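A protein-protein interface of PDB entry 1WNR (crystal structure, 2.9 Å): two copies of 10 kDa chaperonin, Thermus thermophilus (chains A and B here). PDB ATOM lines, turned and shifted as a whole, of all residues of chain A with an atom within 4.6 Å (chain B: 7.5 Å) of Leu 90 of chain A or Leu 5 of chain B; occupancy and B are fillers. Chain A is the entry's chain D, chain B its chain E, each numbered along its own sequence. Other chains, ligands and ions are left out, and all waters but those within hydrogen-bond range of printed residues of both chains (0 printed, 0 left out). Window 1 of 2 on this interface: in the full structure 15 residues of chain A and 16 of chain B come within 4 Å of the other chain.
O of Val 65 of chain A lies within hydrogen-bond range of N of Leu 90 of chain A (2.9 Å).
O of Leu 5 of chain B is in hydrogen-bond range of NE of Arg 8 of chain B, at 2.7 Å.
The backbone carbonyl oxygen (O) of Gly 6 of chain B is in hydrogen-bond range of the backbone NH (N) of Thr 44 of chain B, 3.1 Å away.
O of Gly 6 of chain B is in hydrogen-bond range of N of Gly 45 of chain B (2.9 Å).
The backbone carbonyl oxygen (O) of Arg 8 of chain B lies within hydrogen-bond range of the backbone NH (N) of Gly 43 of chain B.
N of Thr 72 of chain B lies within hydrogen-bond range of O of Ile 83 of chain B (2.8 Å).
Of the printed residues of chain B, Leu 90 of chain A touches Pro 4, Leu 5, Arg 8, Thr 72 and Ile 83.
Of chain A, only Glu 57, Val 58, Leu 89, Leu 90, Ala 91 and Val 92 come within 4 Å of Leu 5 of chain B.
Of the printed residues of chain A, Thr 44 of chain B touches Glu 57 (2.9 Å).
Of the printed residues of chain A, Gly 6 of chain B touches Glu 57.
Ser 85 of chain B touches none of the printed residues of chain A.
Gly 71 of chain B touches none of the printed residues of chain A.
The nearest printed residue of chain B that does not touch Val 92 of chain A is Pro 4 of chain B (5.0 Å).
No position is printed for both chains.
Of the 18 pairs that touch across the chains among the printed residues, none has its exchanged pair printed and touching as well.
Of the 20 printed residues of chain B, 9 touch a printed residue of chain A.
Hydrophobic or aromatic side chains of chain B within 4 Å of the printed part of chain A: Ile 2, Leu 5 and Ile 83.
Along chain B the printed residues that touch a printed residue of chain A span positions 2 to 83.
Among the printed residues, 18 pairs touch across the chains.
Among the printed residues, no Asp or Glu carboxylate lies within 4 Å of a Lys or Arg side-chain nitrogen of the other chain.
N of Gly 6 of chain B lies within hydrogen-bond range of OE2 of Glu 57 of chain A.
The side-chain carboxylate (OE1) of Glu 57 of chain A is in hydrogen-bond range of the side-chain hydroxyl (OG1) of Thr 44 of chain B (2.9 Å).
The guanidinium group of Arg 8 of chain B sits at hydrogen-bond distance from the backbone carbonyl oxygen of Leu 89 of chain A.
The backbone carbonyl oxygen of Leu 90 of chain A is in hydrogen-bond range of the backbone NH of Leu 5 of chain B (2.9 Å).
O of Lys 3 of chain B sits at hydrogen-bond distance from N of Val 92 of chain A (2.8 Å).
Among the printed residues, merely in contact across the chains: Glu 57 of chain A with Leu 5 of chain B (3.6 Å), Val 58 of chain A with Leu 5 of chain B (3.6 Å), Leu 89 of chain A with Leu 5 of chain B (3.7 Å), Leu 90 of chain A with Pro 4 of chain B (3.8 Å), Leu 90 of chain A with Arg 8 of chain B (3.3 Å), Leu 90 of chain A with Thr 72 of chain B (3.9 Å), Leu 90 of chain A with Ile 83 of chain B (3.999 Å), Ala 91 of chain A with Ile 2 of chain B (3.96 Å), Ala 91 of chain A with Lys 3 of chain B (3.0 Å), Ala 91 of chain A with Pro 4 of chain B (3.8 Å), Ala 91 of chain A with Leu 5 of chain B (3.8 Å), Val 92 of chain A with Ile 2 of chain B (3.8 Å) and Val 92 of chain A with Leu 5 of chain B (3.8 Å).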
ATOM      1  N   GLU A  57      30.668 -17.008   4.434  1.00  0.00           N
ATOM      2  CA  GLU A  57      29.590 -17.588   5.230  1.00  0.00           C
ATOM      3  C   GLU A  57      29.911 -19.020   5.706  1.00  0.00           C
ATOM      4  O   GLU A  57      29.029 -19.754   6.139  1.00  0.00           O
ATOM      5  CB  GLU A  57      28.289 -17.554   4.416  1.00  0.00           C
ATOM      6  CG  GLU A  57      27.018 -17.693   5.224  1.00  0.00           C
ATOM      7  CD  GLU A  57      25.789 -17.665   4.347  1.00  0.00           C
ATOM      8  OE1 GLU A  57      24.672 -17.891   4.861  1.00  0.00           O
ATOM      9  OE2 GLU A  57      25.941 -17.419   3.136  1.00  0.00           O
ATOM     10  N   VAL A  58      31.173 -19.423   5.618  1.00  0.00           N
ATOM     11  CA  VAL A  58      31.556 -20.743   6.091  1.00  0.00           C
ATOM     12  C   VAL A  58      32.841 -20.631   6.905  1.00  0.00           C
ATOM     13  O   VAL A  58      33.676 -19.772   6.645  1.00  0.00           O
ATOM     14  CB  VAL A  58      31.741 -21.771   4.924  1.00  0.00           C
ATOM     15  CG1 VAL A  58      30.424 -21.972   4.206  1.00  0.00           C
ATOM     16  CG2 VAL A  58      32.802 -21.309   3.952  1.00  0.00           C
ATOM     17  N   VAL A  65      28.961 -28.447   0.370  1.00  0.00           N
ATOM     18  CA  VAL A  65      28.551 -29.163  -0.822  1.00  0.00           C
ATOM     19  C   VAL A  65      28.852 -28.177  -1.915  1.00  0.00           C
ATOM     20  O   VAL A  65      28.420 -27.023  -1.837  1.00  0.00           O
ATOM     21  CB  VAL A  65      27.022 -29.402  -0.875  1.00  0.00           C
ATOM     22  CG1 VAL A  65      26.630 -30.026  -2.221  1.00  0.00           C
ATOM     23  CG2 VAL A  65      26.590 -30.281   0.256  1.00  0.00           C
ATOM     24  N   PHE A  66      29.579 -28.600  -2.939  1.00  0.00           N
ATOM     25  CA  PHE A  66      29.855 -27.668  -4.021  1.00  0.00           C
ATOM     26  C   PHE A  66      29.608 -28.280  -5.375  1.00  0.00           C
ATOM     27  O   PHE A  66      29.430 -29.484  -5.504  1.00  0.00           O
ATOM     28  CB  PHE A  66      31.286 -27.100  -3.922  1.00  0.00           C
ATOM     29  CG  PHE A  66      32.357 -28.139  -3.823  1.00  0.00           C
ATOM     30  CD1 PHE A  66      33.050 -28.541  -4.942  1.00  0.00           C
ATOM     31  CD2 PHE A  66      32.670 -28.712  -2.601  1.00  0.00           C
ATOM     32  CE1 PHE A  66      34.050 -29.500  -4.853  1.00  0.00           C
ATOM     33  CE2 PHE A  66      33.662 -29.670  -2.503  1.00  0.00           C
ATOM     34  CZ  PHE A  66      34.357 -30.067  -3.635  1.00  0.00           C
ATOM     35  N   ALA A  67      29.572 -27.421  -6.378  1.00  0.00           N
ATOM     36  CA  ALA A  67      29.337 -27.838  -7.746  1.00  0.00           C
ATOM     37  C   ALA A  67      30.406 -28.804  -8.265  1.00  0.00           C
ATOM     38  O   ALA A  67      31.609 -28.598  -8.058  1.00  0.00           O
ATOM     39  CB  ALA A  67      29.271 -26.602  -8.636  1.00  0.00           C
ATOM     40  N   ASP A  88      30.502 -20.653  -5.271  1.00  0.00           N
ATOM     41  CA  ASP A  88      30.410 -22.032  -5.750  1.00  0.00           C
ATOM     42  C   ASP A  88      29.985 -22.995  -4.646  1.00  0.00           C
ATOM     43  O   ASP A  88      29.765 -24.186  -4.888  1.00  0.00           O
ATOM     44  CB  ASP A  88      31.734 -22.480  -6.359  1.00  0.00           C
ATOM     45  CG  ASP A  88      31.851 -22.093  -7.815  1.00  0.00           C
ATOM     46  OD1 ASP A  88      31.468 -20.946  -8.136  1.00  0.00           O
ATOM     47  OD2 ASP A  88      32.320 -22.920  -8.631  1.00  0.00           O
ATOM     48  N   LEU A  89      29.868 -22.459  -3.436  1.00  0.00           N
ATOM     49  CA  LEU A  89      29.439 -23.221  -2.279  1.00  0.00           C
ATOM     50  C   LEU A  89      27.918 -23.192  -2.190  1.00  0.00           C
ATOM     51  O   LEU A  89      27.325 -22.143  -1.937  1.00  0.00           O
ATOM     52  CB  LEU A  89      30.026 -22.615  -1.015  1.00  0.00           C
ATOM     53  CG  LEU A  89      31.538 -22.590  -0.989  1.00  0.00           C
ATOM     54  CD1 LEU A  89      31.996 -21.859   0.277  1.00  0.00           C
ATOM     55  CD2 LEU A  89      32.073 -24.017  -1.067  1.00  0.00           C
ATOM     56  N   LEU A  90      27.303 -24.353  -2.387  1.00  0.00           N
ATOM     57  CA  LEU A  90      25.854 -24.489  -2.345  1.00  0.00           C
ATOM     58  C   LEU A  90      25.256 -24.489  -0.948  1.00  0.00           C
ATOM     59  O   LEU A  90      24.313 -23.746  -0.658  1.00  0.00           O
ATOM     60  CB  LEU A  90      25.444 -25.778  -3.056  1.00  0.00           C
ATOM     61  CG  LEU A  90      25.374 -25.732  -4.578  1.00  0.00           C
ATOM     62  CD1 LEU A  90      26.221 -24.600  -5.113  1.00  0.00           C
ATOM     63  CD2 LEU A  90      25.835 -27.047  -5.126  1.00  0.00           C
ATOM     64  N   ALA A  91      25.799 -25.332  -0.079  1.00  0.00           N
ATOM     65  CA  ALA A  91      25.275 -25.432   1.275  1.00  0.00           C
ATOM     66  C   ALA A  91      26.283 -26.000   2.245  1.00  0.00           C
ATOM     67  O   ALA A  91      27.352 -26.460   1.857  1.00  0.00           O
ATOM     68  CB  ALA A  91      24.029 -26.312   1.273  1.00  0.00           C
ATOM     69  N   VAL A  92      25.927 -25.957   3.520  1.00  0.00           N
ATOM     70  CA  VAL A  92      26.764 -26.513   4.577  1.00  0.00           C
ATOM     71  C   VAL A  92      25.997 -27.706   5.119  1.00  0.00           C
ATOM     72  O   VAL A  92      24.799 -27.599   5.377  1.00  0.00           O
ATOM     73  CB  VAL A  92      26.969 -25.530   5.720  1.00  0.00           C
ATOM     74  CG1 VAL A  92      27.680 -26.202   6.845  1.00  0.00           C
ATOM     75  CG2 VAL A  92      27.768 -24.354   5.230  1.00  0.00           C
ATOM     76  N   ILE B   2      20.710 -29.615   6.220  1.00  0.00           N
ATOM     77  CA  ILE B   2      21.259 -28.941   5.044  1.00  0.00           C
ATOM     78  C   ILE B   2      21.039 -27.428   5.127  1.00  0.00           C
ATOM     79  O   ILE B   2      19.915 -26.947   4.974  1.00  0.00           O
ATOM     80  CB  ILE B   2      20.599 -29.418   3.752  1.00  0.00           C
ATOM     81  CG1 ILE B   2      20.976 -30.865   3.470  1.00  0.00           C
ATOM     82  CG2 ILE B   2      21.049 -28.546   2.605  1.00  0.00           C
ATOM     83  CD1 ILE B   2      20.232 -31.452   2.317  1.00  0.00           C
ATOM     84  N   LYS B   3      22.109 -26.681   5.368  1.00  0.00           N
ATOM     85  CA  LYS B   3      22.002 -25.235   5.471  1.00  0.00           C
ATOM     86  C   LYS B   3      22.332 -24.632   4.107  1.00  0.00           C
ATOM     87  O   LYS B   3      23.490 -24.673   3.674  1.00  0.00           O
ATOM     88  CB  LYS B   3      22.979 -24.725   6.522  1.00  0.00           C
ATOM     89  CG  LYS B   3      22.874 -23.254   6.805  1.00  0.00           C
ATOM     90  CD  LYS B   3      24.090 -22.789   7.591  1.00  0.00           C
ATOM     91  CE  LYS B   3      24.065 -21.289   7.851  1.00  0.00           C
ATOM     92  NZ  LYS B   3      25.370 -20.830   8.398  1.00  0.00           N
ATOM     93  N   PRO B   4      21.322 -24.064   3.410  1.00  0.00           N
ATOM     94  CA  PRO B   4      21.571 -23.470   2.095  1.00  0.00           C
ATOM     95  C   PRO B   4      22.432 -22.228   2.300  1.00  0.00           C
ATOM     96  O   PRO B   4      22.219 -21.478   3.268  1.00  0.00           O
ATOM     97  CB  PRO B   4      20.176 -23.093   1.597  1.00  0.00           C
ATOM     98  CG  PRO B   4      19.216 -23.574   2.654  1.00  0.00           C
ATOM     99  CD  PRO B   4      20.008 -23.635   3.912  1.00  0.00           C
ATOM    100  N   LEU B   5      23.398 -22.007   1.407  1.00  0.00           N
ATOM    101  CA  LEU B   5      24.261 -20.839   1.540  1.00  0.00           C
ATOM    102  C   LEU B   5      23.869 -19.671   0.649  1.00  0.00           C
ATOM    103  O   LEU B   5      23.562 -19.831  -0.539  1.00  0.00           O
ATOM    104  CB  LEU B   5      25.707 -21.216   1.274  1.00  0.00           C
ATOM    105  CG  LEU B   5      26.411 -21.993   2.374  1.00  0.00           C
ATOM    106  CD1 LEU B   5      27.766 -22.395   1.881  1.00  0.00           C
ATOM    107  CD2 LEU B   5      26.525 -21.139   3.630  1.00  0.00           C
ATOM    108  N   GLY B   6      23.852 -18.491   1.256  1.00  0.00           N
ATOM    109  CA  GLY B   6      23.525 -17.293   0.519  1.00  0.00           C
ATOM    110  C   GLY B   6      22.099 -17.168   0.048  1.00  0.00           C
ATOM    111  O   GLY B   6      21.165 -17.353   0.823  1.00  0.00           O
ATOM    112  N   ASP B   7      21.942 -16.844  -1.234  1.00  0.00           N
ATOM    113  CA  ASP B   7      20.636 -16.646  -1.846  1.00  0.00           C
ATOM    114  C   ASP B   7      19.990 -17.936  -2.342  1.00  0.00           C
ATOM    115  O   ASP B   7      19.508 -18.011  -3.470  1.00  0.00           O
ATOM    116  CB  ASP B   7      20.774 -15.672  -3.007  1.00  0.00           C
ATOM    117  CG  ASP B   7      19.444 -15.332  -3.629  1.00  0.00           C
ATOM    118  OD1 ASP B   7      18.584 -14.782  -2.897  1.00  0.00           O
ATOM    119  OD2 ASP B   7      19.251 -15.621  -4.842  1.00  0.00           O
ATOM    120  N   ARG B   8      19.964 -18.949  -1.488  1.00  0.00           N
ATOM    121  CA  ARG B   8      19.387 -20.229  -1.861  1.00  0.00           C
ATOM    122  C   ARG B   8      18.388 -20.776  -0.851  1.00  0.00           C
ATOM    123  O   ARG B   8      18.202 -20.207   0.226  1.00  0.00           O
ATOM    124  CB  ARG B   8      20.516 -21.226  -2.051  1.00  0.00           C
ATOM    125  CG  ARG B   8      21.188 -21.051  -3.365  1.00  0.00           C
ATOM    126  CD  ARG B   8      22.473 -21.827  -3.487  1.00  0.00           C
ATOM    127  NE  ARG B   8      23.586 -21.073  -2.940  1.00  0.00           N
ATOM    128  CZ  ARG B   8      24.765 -20.993  -3.534  1.00  0.00           C
ATOM    129  NH1 ARG B   8      24.951 -21.623  -4.686  1.00  0.00           N
ATOM    130  NH2 ARG B   8      25.752 -20.297  -2.982  1.00  0.00           N
ATOM    131  N   VAL B   9      17.726 -21.866  -1.221  1.00  0.00           N
ATOM    132  CA  VAL B   9      16.790 -22.543  -0.330  1.00  0.00           C
ATOM    133  C   VAL B   9      16.890 -24.023  -0.611  1.00  0.00           C
ATOM    134  O   VAL B   9      17.442 -24.432  -1.639  1.00  0.00           O
ATOM    135  CB  VAL B   9      15.302 -22.132  -0.540  1.00  0.00           C
ATOM    136  CG1 VAL B   9      15.137 -20.653  -0.313  1.00  0.00           C
ATOM    137  CG2 VAL B   9      14.814 -22.559  -1.907  1.00  0.00           C
ATOM    138  N   VAL B  10      16.385 -24.835   0.314  1.00  0.00           N
ATOM    139  CA  VAL B  10      16.385 -26.277   0.102  1.00  0.00           C
ATOM    140  C   VAL B  10      14.922 -26.707   0.060  1.00  0.00           C
ATOM    141  O   VAL B  10      14.121 -26.299   0.900  1.00  0.00           O
ATOM    142  CB  VAL B  10      17.152 -27.036   1.220  1.00  0.00           C
ATOM    143  CG1 VAL B  10      17.083 -28.532   0.980  1.00  0.00           C
ATOM    144  CG2 VAL B  10      18.591 -26.614   1.225  1.00  0.00           C
ATOM    145  N   VAL B  42      15.966 -22.144   4.359  1.00  0.00           N
ATOM    146  CA  VAL B  42      16.228 -20.953   3.558  1.00  0.00           C
ATOM    147  C   VAL B  42      17.550 -20.283   3.913  1.00  0.00           C
ATOM    148  O   VAL B  42      17.933 -20.204   5.075  1.00  0.00           O
ATOM    149  CB  VAL B  42      15.093 -19.935   3.691  1.00  0.00           C
ATOM    150  CG1 VAL B  42      13.769 -20.575   3.277  1.00  0.00           C
ATOM    151  CG2 VAL B  42      15.028 -19.440   5.102  1.00  0.00           C
ATOM    152  N   GLY B  43      18.249 -19.811   2.890  1.00  0.00           N
ATOM    153  CA  GLY B  43      19.527 -19.165   3.104  1.00  0.00           C
ATOM    154  C   GLY B  43      19.359 -17.800   3.728  1.00  0.00           C
ATOM    155  O   GLY B  43      18.251 -17.425   4.092  1.00  0.00           O
ATOM    156  N   THR B  44      20.458 -17.063   3.845  1.00  0.00           N
ATOM    157  CA  THR B  44      20.437 -15.731   4.427  1.00  0.00           C
ATOM    158  C   THR B  44      20.153 -14.634   3.379  1.00  0.00           C
ATOM    159  O   THR B  44      20.053 -13.444   3.705  1.00  0.00           O
ATOM    160  CB  THR B  44      21.768 -15.440   5.167  1.00  0.00           C
ATOM    161  OG1 THR B  44      22.878 -15.705   4.299  1.00  0.00           O
ATOM    162  CG2 THR B  44      21.884 -16.313   6.407  1.00  0.00           C
ATOM    163  N   GLY B  45      20.019 -15.036   2.119  1.00  0.00           N
ATOM    164  CA  GLY B  45      19.718 -14.067   1.084  1.00  0.00           C
ATOM    165  C   GLY B  45      20.916 -13.422   0.429  1.00  0.00           C
ATOM    166  O   GLY B  45      22.040 -13.531   0.901  1.00  0.00           O
ATOM    167  N   GLY B  71      18.214 -26.105 -10.400  1.00  0.00           N
ATOM    168  CA  GLY B  71      18.737 -26.496  -9.104  1.00  0.00           C
ATOM    169  C   GLY B  71      19.773 -27.607  -9.065  1.00  0.00           C
ATOM    170  O   GLY B  71      20.262 -28.071 -10.095  1.00  0.00           O
ATOM    171  N   THR B  72      20.110 -28.029  -7.851  1.00  0.00           N
ATOM    172  CA  THR B  72      21.081 -29.089  -7.641  1.00  0.00           C
ATOM    173  C   THR B  72      20.462 -30.207  -6.813  1.00  0.00           C
ATOM    174  O   THR B  72      19.963 -29.979  -5.715  1.00  0.00           O
ATOM    175  CB  THR B  72      22.309 -28.577  -6.887  1.00  0.00           C
ATOM    176  OG1 THR B  72      22.897 -27.497  -7.606  1.00  0.00           O
ATOM    177  CG2 THR B  72      23.320 -29.667  -6.734  1.00  0.00           C
ATOM    178  N   GLU B  73      20.498 -31.415  -7.355  1.00  0.00           N
ATOM    179  CA  GLU B  73      19.970 -32.594  -6.688  1.00  0.00           C
ATOM    180  C   GLU B  73      21.028 -33.123  -5.729  1.00  0.00           C
ATOM    181  O   GLU B  73      22.172 -33.349  -6.118  1.00  0.00           O
ATOM    182  CB  GLU B  73      19.675 -33.669  -7.716  1.00  0.00           C
ATOM    183  CG  GLU B  73      18.547 -33.351  -8.642  1.00  0.00           C
ATOM    184  CD  GLU B  73      17.247 -33.921  -8.141  1.00  0.00           C
ATOM    185  OE1 GLU B  73      16.221 -33.743  -8.842  1.00  0.00           O
ATOM    186  OE2 GLU B  73      17.258 -34.552  -7.049  1.00  0.00           O
ATOM    187  N   ILE B  74      20.650 -33.328  -4.478  1.00  0.00           N
ATOM    188  CA  ILE B  74      21.578 -33.836  -3.486  1.00  0.00           C
ATOM    189  C   ILE B  74      20.856 -34.940  -2.755  1.00  0.00           C
ATOM    190  O   ILE B  74      19.657 -34.845  -2.504  1.00  0.00           O
ATOM    191  CB  ILE B  74      21.978 -32.728  -2.477  1.00  0.00           C
ATOM    192  CG1 ILE B  74      22.848 -33.297  -1.367  1.00  0.00           C
ATOM    193  CG2 ILE B  74      20.741 -32.121  -1.860  1.00  0.00           C
ATOM    194  CD1 ILE B  74      24.134 -33.849  -1.846  1.00  0.00           C
ATOM    195  N   ILE B  83      18.614 -28.119  -4.051  1.00  0.00           N
ATOM    196  CA  ILE B  83      19.132 -26.827  -3.640  1.00  0.00           C
ATOM    197  C   ILE B  83      18.872 -25.888  -4.818  1.00  0.00           C
ATOM    198  O   ILE B  83      19.357 -26.125  -5.918  1.00  0.00           O
ATOM    199  CB  ILE B  83      20.641 -26.886  -3.346  1.00  0.00           C
ATOM    200  CG1 ILE B  83      20.921 -27.883  -2.222  1.00  0.00           C
ATOM    201  CG2 ILE B  83      21.138 -25.509  -2.940  1.00  0.00           C
ATOM    202  CD1 ILE B  83      22.397 -28.141  -1.996  1.00  0.00           C
ATOM    203  N   LEU B  84      18.075 -24.851  -4.576  1.00  0.00           N
ATOM    204  CA  LEU B  84      17.723 -23.856  -5.582  1.00  0.00           C
ATOM    205  C   LEU B  84      18.047 -22.451  -5.077  1.00  0.00           C
ATOM    206  O   LEU B  84      17.955 -22.178  -3.876  1.00  0.00           O
ATOM    207  CB  LEU B  84      16.230 -23.919  -5.880  1.00  0.00           C
ATOM    208  CG  LEU B  84      15.707 -25.187  -6.535  1.00  0.00           C
ATOM    209  CD1 LEU B  84      14.220 -25.282  -6.314  1.00  0.00           C
ATOM    210  CD2 LEU B  84      16.034 -25.185  -8.008  1.00  0.00           C
ATOM    211  N   SER B  85      18.438 -21.559  -5.989  1.00  0.00           N
ATOM    212  CA  SER B  85      18.713 -20.175  -5.604  1.00  0.00           C
ATOM    213  C   SER B  85      17.435 -19.371  -5.858  1.00  0.00           C
ATOM    214  O   SER B  85      16.620 -19.725  -6.711  1.00  0.00           O
ATOM    215  CB  SER B  85      19.874 -19.602  -6.406  1.00  0.00           C
ATOM    216  OG  SER B  85      19.739 -19.950  -7.764  1.00  0.00           O
